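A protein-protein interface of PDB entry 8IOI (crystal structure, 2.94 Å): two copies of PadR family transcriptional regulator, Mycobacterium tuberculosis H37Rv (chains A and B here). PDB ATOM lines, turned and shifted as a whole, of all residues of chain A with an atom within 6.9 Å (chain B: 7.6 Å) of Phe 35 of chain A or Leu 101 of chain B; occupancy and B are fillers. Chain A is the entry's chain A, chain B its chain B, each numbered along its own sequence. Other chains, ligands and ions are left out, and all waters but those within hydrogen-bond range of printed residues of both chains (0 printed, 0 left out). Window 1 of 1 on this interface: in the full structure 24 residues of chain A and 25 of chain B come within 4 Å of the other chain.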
ATOM      1  N   ALA A   9       5.749   6.499  31.062  1.00  0.00           N
ATOM      2  CA  ALA A   9       6.850   7.380  30.718  1.00  0.00           C
ATOM      3  C   ALA A   9       6.979   8.435  31.804  1.00  0.00           C
ATOM      4  O   ALA A   9       8.087   8.791  32.184  1.00  0.00           O
ATOM      5  CB  ALA A   9       6.604   8.007  29.368  1.00  0.00           C
ATOM      6  N   PHE A  28      10.629  16.416  30.579  1.00  0.00           N
ATOM      7  CA  PHE A  28      10.206  15.340  29.693  1.00  0.00           C
ATOM      8  C   PHE A  28      10.672  15.648  28.270  1.00  0.00           C
ATOM      9  O   PHE A  28      11.108  14.761  27.533  1.00  0.00           O
ATOM     10  CB  PHE A  28       8.684  15.186  29.761  1.00  0.00           C
ATOM     11  CG  PHE A  28       8.082  14.060  28.958  1.00  0.00           C
ATOM     12  CD1 PHE A  28       7.866  14.203  27.592  1.00  0.00           C
ATOM     13  CD2 PHE A  28       7.691  12.878  29.578  1.00  0.00           C
ATOM     14  CE1 PHE A  28       7.296  13.172  26.864  1.00  0.00           C
ATOM     15  CE2 PHE A  28       7.107  11.852  28.849  1.00  0.00           C
ATOM     16  CZ  PHE A  28       6.917  12.002  27.492  1.00  0.00           C
ATOM     17  N   ASP A  29      10.576  16.928  27.905  1.00  0.00           N
ATOM     18  CA  ASP A  29      10.929  17.380  26.575  1.00  0.00           C
ATOM     19  C   ASP A  29      12.438  17.258  26.387  1.00  0.00           C
ATOM     20  O   ASP A  29      12.913  16.919  25.301  1.00  0.00           O
ATOM     21  CB  ASP A  29      10.452  18.813  26.363  1.00  0.00           C
ATOM     22  CG  ASP A  29       8.957  18.945  26.154  1.00  0.00           C
ATOM     23  OD1 ASP A  29       8.257  17.899  26.097  1.00  0.00           O
ATOM     24  OD2 ASP A  29       8.513  20.098  26.018  1.00  0.00           O
ATOM     25  N   SER A  31      14.447  15.169  27.948  1.00  0.00           N
ATOM     26  CA  SER A  31      14.928  13.795  28.041  1.00  0.00           C
ATOM     27  C   SER A  31      14.115  12.865  27.140  1.00  0.00           C
ATOM     28  O   SER A  31      14.622  12.396  26.119  1.00  0.00           O
ATOM     29  CB  SER A  31      14.944  13.299  29.461  1.00  0.00           C
ATOM     30  OG  SER A  31      13.615  13.221  29.960  1.00  0.00           O
ATOM     31  N   ILE A  32      12.856  12.605  27.513  1.00  0.00           N
ATOM     32  CA  ILE A  32      12.084  11.544  26.879  1.00  0.00           C
ATOM     33  C   ILE A  32      11.389  12.080  25.626  1.00  0.00           C
ATOM     34  O   ILE A  32      10.910  11.300  24.809  1.00  0.00           O
ATOM     35  CB  ILE A  32      11.130  10.850  27.874  1.00  0.00           C
ATOM     36  CG1 ILE A  32      11.915  10.150  28.987  1.00  0.00           C
ATOM     37  CG2 ILE A  32      10.198   9.884  27.153  1.00  0.00           C
ATOM     38  CD1 ILE A  32      11.235  10.172  30.343  1.00  0.00           C
ATOM     39  N   GLY A  33      11.417  13.405  25.444  1.00  0.00           N
ATOM     40  CA  GLY A  33      10.827  14.058  24.287  1.00  0.00           C
ATOM     41  C   GLY A  33      11.613  13.830  22.995  1.00  0.00           C
ATOM     42  O   GLY A  33      11.101  14.115  21.915  1.00  0.00           O
ATOM     43  N   TYR A  34      12.852  13.329  23.107  1.00  0.00           N
ATOM     44  CA  TYR A  34      13.686  13.028  21.954  1.00  0.00           C
ATOM     45  C   TYR A  34      13.317  11.671  21.345  1.00  0.00           C
ATOM     46  O   TYR A  34      13.874  11.289  20.322  1.00  0.00           O
ATOM     47  CB  TYR A  34      15.169  13.014  22.331  1.00  0.00           C
ATOM     48  CG  TYR A  34      15.870  14.350  22.393  1.00  0.00           C
ATOM     49  CD1 TYR A  34      16.370  14.962  21.246  1.00  0.00           C
ATOM     50  CD2 TYR A  34      16.080  14.986  23.611  1.00  0.00           C
ATOM     51  CE1 TYR A  34      17.024  16.187  21.307  1.00  0.00           C
ATOM     52  CE2 TYR A  34      16.731  16.210  23.689  1.00  0.00           C
ATOM     53  CZ  TYR A  34      17.203  16.812  22.534  1.00  0.00           C
ATOM     54  OH  TYR A  34      17.849  18.012  22.622  1.00  0.00           O
ATOM     55  N   PHE A  35      12.410  10.924  21.985  1.00  0.00           N
ATOM     56  CA  PHE A  35      11.892   9.700  21.392  1.00  0.00           C
ATOM     57  C   PHE A  35      10.362   9.702  21.409  1.00  0.00           C
ATOM     58  O   PHE A  35       9.711   8.998  20.641  1.00  0.00           O
ATOM     59  CB  PHE A  35      12.568   8.452  21.974  1.00  0.00           C
ATOM     60  CG  PHE A  35      12.720   8.360  23.473  1.00  0.00           C
ATOM     61  CD1 PHE A  35      13.818   8.908  24.124  1.00  0.00           C
ATOM     62  CD2 PHE A  35      11.814   7.633  24.235  1.00  0.00           C
ATOM     63  CE1 PHE A  35      13.975   8.780  25.499  1.00  0.00           C
ATOM     64  CE2 PHE A  35      11.976   7.499  25.609  1.00  0.00           C
ATOM     65  CZ  PHE A  35      13.056   8.069  26.240  1.00  0.00           C
ATOM     66  N   TRP A  36       9.799  10.534  22.283  1.00  0.00           N
ATOM     67  CA  TRP A  36       8.373  10.659  22.520  1.00  0.00           C
ATOM     68  C   TRP A  36       7.914  12.073  22.172  1.00  0.00           C
ATOM     69  O   TRP A  36       8.412  13.057  22.723  1.00  0.00           O
ATOM     70  CB  TRP A  36       8.142  10.441  24.011  1.00  0.00           C
ATOM     71  CG  TRP A  36       7.519   9.153  24.428  1.00  0.00           C
ATOM     72  CD1 TRP A  36       8.157   7.989  24.749  1.00  0.00           C
ATOM     73  CD2 TRP A  36       6.122   8.929  24.657  1.00  0.00           C
ATOM     74  NE1 TRP A  36       7.247   7.041  25.132  1.00  0.00           N
ATOM     75  CE2 TRP A  36       5.992   7.592  25.086  1.00  0.00           C
ATOM     76  CE3 TRP A  36       4.977   9.721  24.522  1.00  0.00           C
ATOM     77  CZ2 TRP A  36       4.751   7.033  25.384  1.00  0.00           C
ATOM     78  CZ3 TRP A  36       3.751   9.167  24.815  1.00  0.00           C
ATOM     79  CH2 TRP A  36       3.646   7.840  25.236  1.00  0.00           C
ATOM     80  N   THR A  37       6.932  12.175  21.280  1.00  0.00           N
ATOM     81  CA  THR A  37       6.284  13.449  21.037  1.00  0.00           C
ATOM     82  C   THR A  37       4.980  13.453  21.822  1.00  0.00           C
ATOM     83  O   THR A  37       4.048  12.738  21.470  1.00  0.00           O
ATOM     84  CB  THR A  37       6.025  13.643  19.542  1.00  0.00           C
ATOM     85  OG1 THR A  37       5.613  12.369  19.043  1.00  0.00           O
ATOM     86  CG2 THR A  37       7.250  14.110  18.788  1.00  0.00           C
ATOM     87  N   THR A 106      10.457  -0.096  20.264  1.00  0.00           N
ATOM     88  CA  THR A 106      11.773   0.504  20.379  1.00  0.00           C
ATOM     89  C   THR A 106      11.732   1.580  21.467  1.00  0.00           C
ATOM     90  O   THR A 106      12.632   1.675  22.293  1.00  0.00           O
ATOM     91  CB  THR A 106      12.258   0.939  18.986  1.00  0.00           C
ATOM     92  OG1 THR A 106      12.188  -0.187  18.112  1.00  0.00           O
ATOM     93  CG2 THR A 106      13.685   1.434  18.960  1.00  0.00           C
ATOM     94  N   ARG A 107      10.643   2.352  21.475  1.00  0.00           N
ATOM     95  CA  ARG A 107      10.424   3.485  22.355  1.00  0.00           C
ATOM     96  C   ARG A 107      10.058   2.994  23.749  1.00  0.00           C
ATOM     97  O   ARG A 107      10.503   3.571  24.739  1.00  0.00           O
ATOM     98  CB  ARG A 107       9.265   4.293  21.766  1.00  0.00           C
ATOM     99  CG  ARG A 107       8.964   5.621  22.443  1.00  0.00           C
ATOM    100  CD  ARG A 107       7.577   5.893  21.933  1.00  0.00           C
ATOM    101  NE  ARG A 107       6.701   4.997  22.662  1.00  0.00           N
ATOM    102  CZ  ARG A 107       5.381   5.039  22.604  1.00  0.00           C
ATOM    103  NH1 ARG A 107       4.779   5.951  21.859  1.00  0.00           N
ATOM    104  NH2 ARG A 107       4.662   4.185  23.313  1.00  0.00           N
ATOM    105  N   ASP A 108       9.237   1.937  23.805  1.00  0.00           N
ATOM    106  CA  ASP A 108       8.774   1.354  25.056  1.00  0.00           C
ATOM    107  C   ASP A 108       9.964   0.777  25.814  1.00  0.00           C
ATOM    108  O   ASP A 108      10.051   0.923  27.030  1.00  0.00           O
ATOM    109  CB  ASP A 108       7.713   0.281  24.819  1.00  0.00           C
ATOM    110  CG  ASP A 108       6.406   0.848  24.291  1.00  0.00           C
ATOM    111  OD1 ASP A 108       6.219   2.067  24.413  1.00  0.00           O
ATOM    112  OD2 ASP A 108       5.592   0.075  23.757  1.00  0.00           O
ATOM    113  N   ALA A 110      12.996   1.802  25.517  1.00  0.00           N
ATOM    114  CA  ALA A 110      13.854   2.897  25.928  1.00  0.00           C
ATOM    115  C   ALA A 110      13.377   3.424  27.275  1.00  0.00           C
ATOM    116  O   ALA A 110      14.197   3.760  28.130  1.00  0.00           O
ATOM    117  CB  ALA A 110      13.865   3.982  24.885  1.00  0.00           C
ATOM    118  N   VAL A 111      12.046   3.471  27.441  1.00  0.00           N
ATOM    119  CA  VAL A 111      11.437   3.977  28.660  1.00  0.00           C
ATOM    120  C   VAL A 111      11.688   2.962  29.767  1.00  0.00           C
ATOM    121  O   VAL A 111      12.113   3.327  30.856  1.00  0.00           O
ATOM    122  CB  VAL A 111       9.927   4.274  28.509  1.00  0.00           C
ATOM    123  CG1 VAL A 111       9.288   4.607  29.846  1.00  0.00           C
ATOM    124  CG2 VAL A 111       9.624   5.384  27.507  1.00  0.00           C
ATOM    125  N   ARG A 114      15.166   3.028  31.010  1.00  0.00           N
ATOM    126  CA  ARG A 114      15.442   4.152  31.890  1.00  0.00           C
ATOM    127  C   ARG A 114      15.134   3.763  33.334  1.00  0.00           C
ATOM    128  O   ARG A 114      16.041   3.631  34.155  1.00  0.00           O
ATOM    129  CB  ARG A 114      14.639   5.389  31.487  1.00  0.00           C
ATOM    130  CG  ARG A 114      15.451   6.387  30.676  1.00  0.00           C
ATOM    131  CD  ARG A 114      14.799   7.759  30.705  1.00  0.00           C
ATOM    132  NE  ARG A 114      15.361   8.617  29.675  1.00  0.00           N
ATOM    133  CZ  ARG A 114      16.215   9.595  29.916  1.00  0.00           C
ATOM    134  NH1 ARG A 114      16.689  10.315  28.912  1.00  0.00           N
ATOM    135  NH2 ARG A 114      16.593   9.850  31.160  1.00  0.00           N
ATOM    136  N   GLY B  96       7.533  17.794  15.238  1.00  0.00           N
ATOM    137  CA  GLY B  96       8.509  16.812  15.691  1.00  0.00           C
ATOM    138  C   GLY B  96       9.959  17.232  15.457  1.00  0.00           C
ATOM    139  O   GLY B  96      10.858  16.414  15.642  1.00  0.00           O
ATOM    140  N   GLY B  98      13.697  18.355  15.614  1.00  0.00           N
ATOM    141  CA  GLY B  98      14.742  18.304  16.617  1.00  0.00           C
ATOM    142  C   GLY B  98      15.242  16.895  16.906  1.00  0.00           C
ATOM    143  O   GLY B  98      16.217  16.761  17.642  1.00  0.00           O
ATOM    144  N   SER B  99      14.605  15.859  16.332  1.00  0.00           N
ATOM    145  CA  SER B  99      15.061  14.485  16.532  1.00  0.00           C
ATOM    146  C   SER B  99      14.658  13.570  15.377  1.00  0.00           C
ATOM    147  O   SER B  99      13.582  13.709  14.807  1.00  0.00           O
ATOM    148  CB  SER B  99      14.547  13.927  17.833  1.00  0.00           C
ATOM    149  OG  SER B  99      14.892  12.557  17.965  1.00  0.00           O
ATOM    150  N   ALA B 100      15.511  12.583  15.095  1.00  0.00           N
ATOM    151  CA  ALA B 100      15.274  11.618  14.038  1.00  0.00           C
ATOM    152  C   ALA B 100      14.129  10.686  14.425  1.00  0.00           C
ATOM    153  O   ALA B 100      13.519  10.063  13.561  1.00  0.00           O
ATOM    154  CB  ALA B 100      16.541  10.840  13.800  1.00  0.00           C
ATOM    155  N   LEU B 101      13.863  10.584  15.729  1.00  0.00           N
ATOM    156  CA  LEU B 101      12.881   9.648  16.241  1.00  0.00           C
ATOM    157  C   LEU B 101      11.523  10.334  16.277  1.00  0.00           C
ATOM    158  O   LEU B 101      10.496   9.668  16.354  1.00  0.00           O
ATOM    159  CB  LEU B 101      13.320   9.171  17.626  1.00  0.00           C
ATOM    160  CG  LEU B 101      14.671   8.443  17.668  1.00  0.00           C
ATOM    161  CD1 LEU B 101      15.155   8.232  19.090  1.00  0.00           C
ATOM    162  CD2 LEU B 101      14.626   7.113  16.936  1.00  0.00           C
ATOM    163  N   THR B 102      11.530  11.667  16.198  1.00  0.00           N
ATOM    164  CA  THR B 102      10.287  12.402  16.363  1.00  0.00           C
ATOM    165  C   THR B 102       9.952  13.164  15.088  1.00  0.00           C
ATOM    166  O   THR B 102       8.785  13.406  14.802  1.00  0.00           O
ATOM    167  CB  THR B 102      10.307  13.237  17.648  1.00  0.00           C
ATOM    168  OG1 THR B 102      11.403  14.157  17.639  1.00  0.00           O
ATOM    169  CG2 THR B 102      10.374  12.379  18.892  1.00  0.00           C
ATOM    170  N   ASP B 103      10.988  13.495  14.317  1.00  0.00           N
ATOM    171  CA  ASP B 103      10.840  14.287  13.107  1.00  0.00           C
ATOM    172  C   ASP B 103      10.217  13.443  12.007  1.00  0.00           C
ATOM    173  O   ASP B 103      10.646  12.324  11.748  1.00  0.00           O
ATOM    174  CB  ASP B 103      12.187  14.851  12.674  1.00  0.00           C
ATOM    175  CG  ASP B 103      12.094  16.043  11.745  1.00  0.00           C
ATOM    176  OD1 ASP B 103      11.077  16.153  11.043  1.00  0.00           O
ATOM    177  OD2 ASP B 103      13.062  16.839  11.718  1.00  0.00           O
ATOM    178  N   SER B 104       9.229  14.017  11.330  1.00  0.00           N
ATOM    179  CA  SER B 104       8.441  13.266  10.368  1.00  0.00           C
ATOM    180  C   SER B 104       8.905  13.568   8.947  1.00  0.00           C
ATOM    181  O   SER B 104       8.237  13.207   7.976  1.00  0.00           O
ATOM    182  CB  SER B 104       6.978  13.579  10.529  1.00  0.00           C
ATOM    183  OG  SER B 104       6.703  14.933  10.170  1.00  0.00           O
ATOM    184  N   THR B 106      11.694  12.525   7.626  1.00  0.00           N
ATOM    185  CA  THR B 106      12.308  11.328   7.086  1.00  0.00           C
ATOM    186  C   THR B 106      11.257  10.536   6.310  1.00  0.00           C
ATOM    187  O   THR B 106      11.539  10.025   5.226  1.00  0.00           O
ATOM    188  CB  THR B 106      13.069  10.567   8.173  1.00  0.00           C
ATOM    189  OG1 THR B 106      14.348  10.362   7.585  1.00  0.00           O
ATOM    190  CG2 THR B 106      12.455   9.236   8.538  1.00  0.00           C
ATOM    191  N   ARG B 135      19.967  17.060  11.088  1.00  0.00           N
ATOM    192  CA  ARG B 135      20.330  15.850  11.801  1.00  0.00           C
ATOM    193  C   ARG B 135      21.707  16.019  12.443  1.00  0.00           C
ATOM    194  O   ARG B 135      21.990  15.432  13.487  1.00  0.00           O
ATOM    195  CB  ARG B 135      20.266  14.651  10.853  1.00  0.00           C
ATOM    196  CG  ARG B 135      18.854  14.231  10.464  1.00  0.00           C
ATOM    197  CD  ARG B 135      18.026  13.650  11.609  1.00  0.00           C
ATOM    198  NE  ARG B 135      17.576  14.699  12.514  1.00  0.00           N
ATOM    199  CZ  ARG B 135      16.459  15.409  12.353  1.00  0.00           C
ATOM    200  NH1 ARG B 135      15.645  15.163  11.339  1.00  0.00           N
ATOM    201  NH2 ARG B 135      16.143  16.362  13.218  1.00  0.00           N
ATOM    202  N   TYR B 142      23.551  15.820  20.831  1.00  0.00           N
ATOM    203  CA  TYR B 142      23.651  14.565  21.552  1.00  0.00           C
ATOM    204  C   TYR B 142      25.112  14.291  21.873  1.00  0.00           C
ATOM    205  O   TYR B 142      25.435  13.724  22.919  1.00  0.00           O
ATOM    206  CB  TYR B 142      23.230  13.404  20.649  1.00  0.00           C
ATOM    207  CG  TYR B 142      21.761  13.081  20.592  1.00  0.00           C
ATOM    208  CD1 TYR B 142      21.002  12.969  21.740  1.00  0.00           C
ATOM    209  CD2 TYR B 142      21.142  12.814  19.387  1.00  0.00           C
ATOM    210  CE1 TYR B 142      19.659  12.629  21.690  1.00  0.00           C
ATOM    211  CE2 TYR B 142      19.804  12.469  19.319  1.00  0.00           C
ATOM    212  CZ  TYR B 142      19.057  12.374  20.472  1.00  0.00           C
ATOM    213  OH  TYR B 142      17.743  12.025  20.360  1.00  0.00           O
ATOM    214  N   VAL B 166      20.313   4.872  26.318  1.00  0.00           N
ATOM    215  CA  VAL B 166      19.150   5.474  25.689  1.00  0.00           C
ATOM    216  C   VAL B 166      19.615   6.596  24.773  1.00  0.00           C
ATOM    217  O   VAL B 166      19.081   6.758  23.679  1.00  0.00           O
ATOM    218  CB  VAL B 166      18.120   5.964  26.720  1.00  0.00           C
ATOM    219  CG1 VAL B 166      17.106   6.910  26.100  1.00  0.00           C
ATOM    220  CG2 VAL B 166      17.418   4.788  27.378  1.00  0.00           C
ATOM    221  N   LEU B 167      20.626   7.344  25.233  1.00  0.00           N
ATOM    222  CA  LEU B 167      21.224   8.428  24.466  1.00  0.00           C
ATOM    223  C   LEU B 167      21.911   7.856  23.235  1.00  0.00           C
ATOM    224  O   LEU B 167      21.935   8.484  22.182  1.00  0.00           O
ATOM    225  CB  LEU B 167      22.243   9.151  25.344  1.00  0.00           C
ATOM    226  CG  LEU B 167      22.890  10.372  24.698  1.00  0.00           C
ATOM    227  CD1 LEU B 167      21.863  11.475  24.523  1.00  0.00           C
ATOM    228  CD2 LEU B 167      24.037  10.880  25.555  1.00  0.00           C
ATOM    229  N   GLY B 169      20.898   5.303  21.629  1.00  0.00           N
ATOM    230  CA  GLY B 169      19.885   4.956  20.639  1.00  0.00           C
ATOM    231  C   GLY B 169      19.555   6.151  19.745  1.00  0.00           C
ATOM    232  O   GLY B 169      19.371   6.018  18.532  1.00  0.00           O
ATOM    233  N   GLY B 170      19.500   7.328  20.377  1.00  0.00           N
ATOM    234  CA  GLY B 170      19.255   8.572  19.674  1.00  0.00           C
ATOM    235  C   GLY B 170      20.441   8.939  18.791  1.00  0.00           C
ATOM    236  O   GLY B 170      20.257   9.436  17.677  1.00  0.00           O
ATOM    237  N   ILE B 171      21.648   8.657  19.305  1.00  0.00           N
ATOM    238  CA  ILE B 171      22.883   8.924  18.584  1.00  0.00           C
ATOM    239  C   ILE B 171      22.930   8.066  17.318  1.00  0.00           C
ATOM    240  O   ILE B 171      23.354   8.525  16.259  1.00  0.00           O
ATOM    241  CB  ILE B 171      24.121   8.709  19.475  1.00  0.00           C
ATOM    242  CG1 ILE B 171      24.314   9.858  20.462  1.00  0.00           C
ATOM    243  CG2 ILE B 171      25.364   8.522  18.622  1.00  0.00           C
ATOM    244  CD1 ILE B 171      25.689   9.858  21.066  1.00  0.00           C
ATOM    245  N   ARG B 172      22.467   6.820  17.432  1.00  0.00           N
ATOM    246  CA  ARG B 172      22.484   5.892  16.317  1.00  0.00           C
ATOM    247  C   ARG B 172      21.487   6.335  15.255  1.00  0.00           C
ATOM    248  O   ARG B 172      21.784   6.263  14.060  1.00  0.00           O
ATOM    249  CB  ARG B 172      22.150   4.479  16.789  1.00  0.00           C
ATOM    250  CG  ARG B 172      23.248   3.842  17.630  1.00  0.00           C
ATOM    251  CD  ARG B 172      22.891   2.434  18.074  1.00  0.00           C
ATOM    252  NE  ARG B 172      24.107   1.644  18.201  1.00  0.00           N
ATOM    253  CZ  ARG B 172      24.709   1.037  17.185  1.00  0.00           C
ATOM    254  NH1 ARG B 172      24.208   1.114  15.960  1.00  0.00           N
ATOM    255  NH2 ARG B 172      25.822   0.363  17.408  1.00  0.00           N
ATOM    256  N   ALA B 173      20.301   6.763  15.706  1.00  0.00           N
ATOM    257  CA  ALA B 173      19.227   7.154  14.809  1.00  0.00           C
ATOM    258  C   ALA B 173      19.670   8.347  13.973  1.00  0.00           C
ATOM    259  O   ALA B 173      19.418   8.380  12.771  1.00  0.00           O
ATOM    260  CB  ALA B 173      17.987   7.484  15.592  1.00  0.00           C
ATOM    261  N   GLU B 174      20.342   9.306  14.625  1.00  0.00           N
ATOM    262  CA  GLU B 174      20.789  10.510  13.952  1.00  0.00           C
ATOM    263  C   GLU B 174      21.802  10.137  12.883  1.00  0.00           C
ATOM    264  O   GLU B 174      21.760  10.661  11.771  1.00  0.00           O
ATOM    265  CB  GLU B 174      21.371  11.506  14.951  1.00  0.00           C
ATOM    266  CG  GLU B 174      20.337  12.001  15.947  1.00  0.00           C
ATOM    267  CD  GLU B 174      19.170  12.816  15.395  1.00  0.00           C
ATOM    268  OE1 GLU B 174      18.241  13.147  16.182  1.00  0.00           O
ATOM    269  OE2 GLU B 174      19.191  13.144  14.187  1.00  0.00           O
ATOM    270  N   ALA B 177      20.046   8.348   9.993  1.00  0.00           N
ATOM    271  CA  ALA B 177      19.312   9.287   9.160  1.00  0.00           C
ATOM    272  C   ALA B 177      20.266   9.987   8.202  1.00  0.00           C
ATOM    273  O   ALA B 177      19.963  10.103   7.011  1.00  0.00           O
ATOM    274  CB  ALA B 177      18.572  10.287  10.013  1.00  0.00           C
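Of the 16 printed residues of chain A, 6 touch a printed residue of chain B.
Hydrophobic or aromatic side chains of chain A within 4 Å of the printed part of chain B: Tyr 34 and Phe 35.
Printed residues of chain B that touch a printed residue of chain A: Gly 98, Ser 99, Leu 101, Thr 102, Tyr 142 and Val 166.
Hydrophobic or aromatic side chains of chain B that line the printed part of chain A: Leu 101, Tyr 142 and Val 166.
Among the printed residues, 12 pairs touch across the chains.
The side-chain hydroxyl (OG) of Ser 99 of chain B sits at hydrogen-bond distance from the backbone carbonyl oxygen (O) of Tyr 34 of chain A (2.9 Å).
Printed residues of chain B within 4 Å of Phe 35 of chain A: Leu 101, Thr 102 and Val 166.
Leu 101 of chain B touches two residues of chain A.
Of the printed residues of chain B, Ala 110 of chain A touches Val 166.
Of the printed residues of chain B, Gly 33 of chain A touches Thr 102.
Of the printed residues of chain B, Trp 36 of chain A touches Thr 102.
Printed residues of chain A within 4 Å of Thr 102 of chain B: Gly 33 (3.6 Å), Tyr 34 (3.9 Å), Phe 35 (3.7 Å), Trp 36 (3.9 Å) and Thr 37 (3.4 Å).
Of the printed residues of chain A, Gly 98 of chain B touches Tyr 34.
The nearest residue of chain B that does not touch Phe 35 of chain A is Ser 99 of chain B (5.0 Å).
Position printed for both chains: 106.
Of the 12 pairs that touch across the chains among the printed residues, none has its exchanged pair printed and touching as well.
Among the printed residues, merely in contact across the chains: Gly 33 of chain A with Thr 102 of chain B, Tyr 34 of chain A with Gly 98 of chain B, Tyr 34 of chain A with Leu 101 of chain B, Tyr 34 of chain A with Thr 102 of chain B, Tyr 34 of chain A with Tyr 142 of chain B, Phe 35 of chain A with Leu 101 of chain B, Phe 35 of chain A with Thr 102 of chain B, Phe 35 of chain A with Val 166 of chain B, Trp 36 of chain A with Thr 102 of chain B, Thr 37 of chain A with Thr 102 of chain B and Ala 110 of chain A with Val 166 of chain B.
The backbone NH (N) of Gly 33 of chain A is in hydrogen-bond range of the backbone carbonyl oxygen (O) of Phe 28 of chain A.
The backbone carbonyl oxygen (O) of Gly 96 of chain B sits at hydrogen-bond distance from the side-chain hydroxyl (OG1) of Thr 102 of chain B (3.1 Å).
The backbone NH of Leu 101 of chain B lies close to the side-chain hydroxyl of Ser 99 of chain B (3.2 Å).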
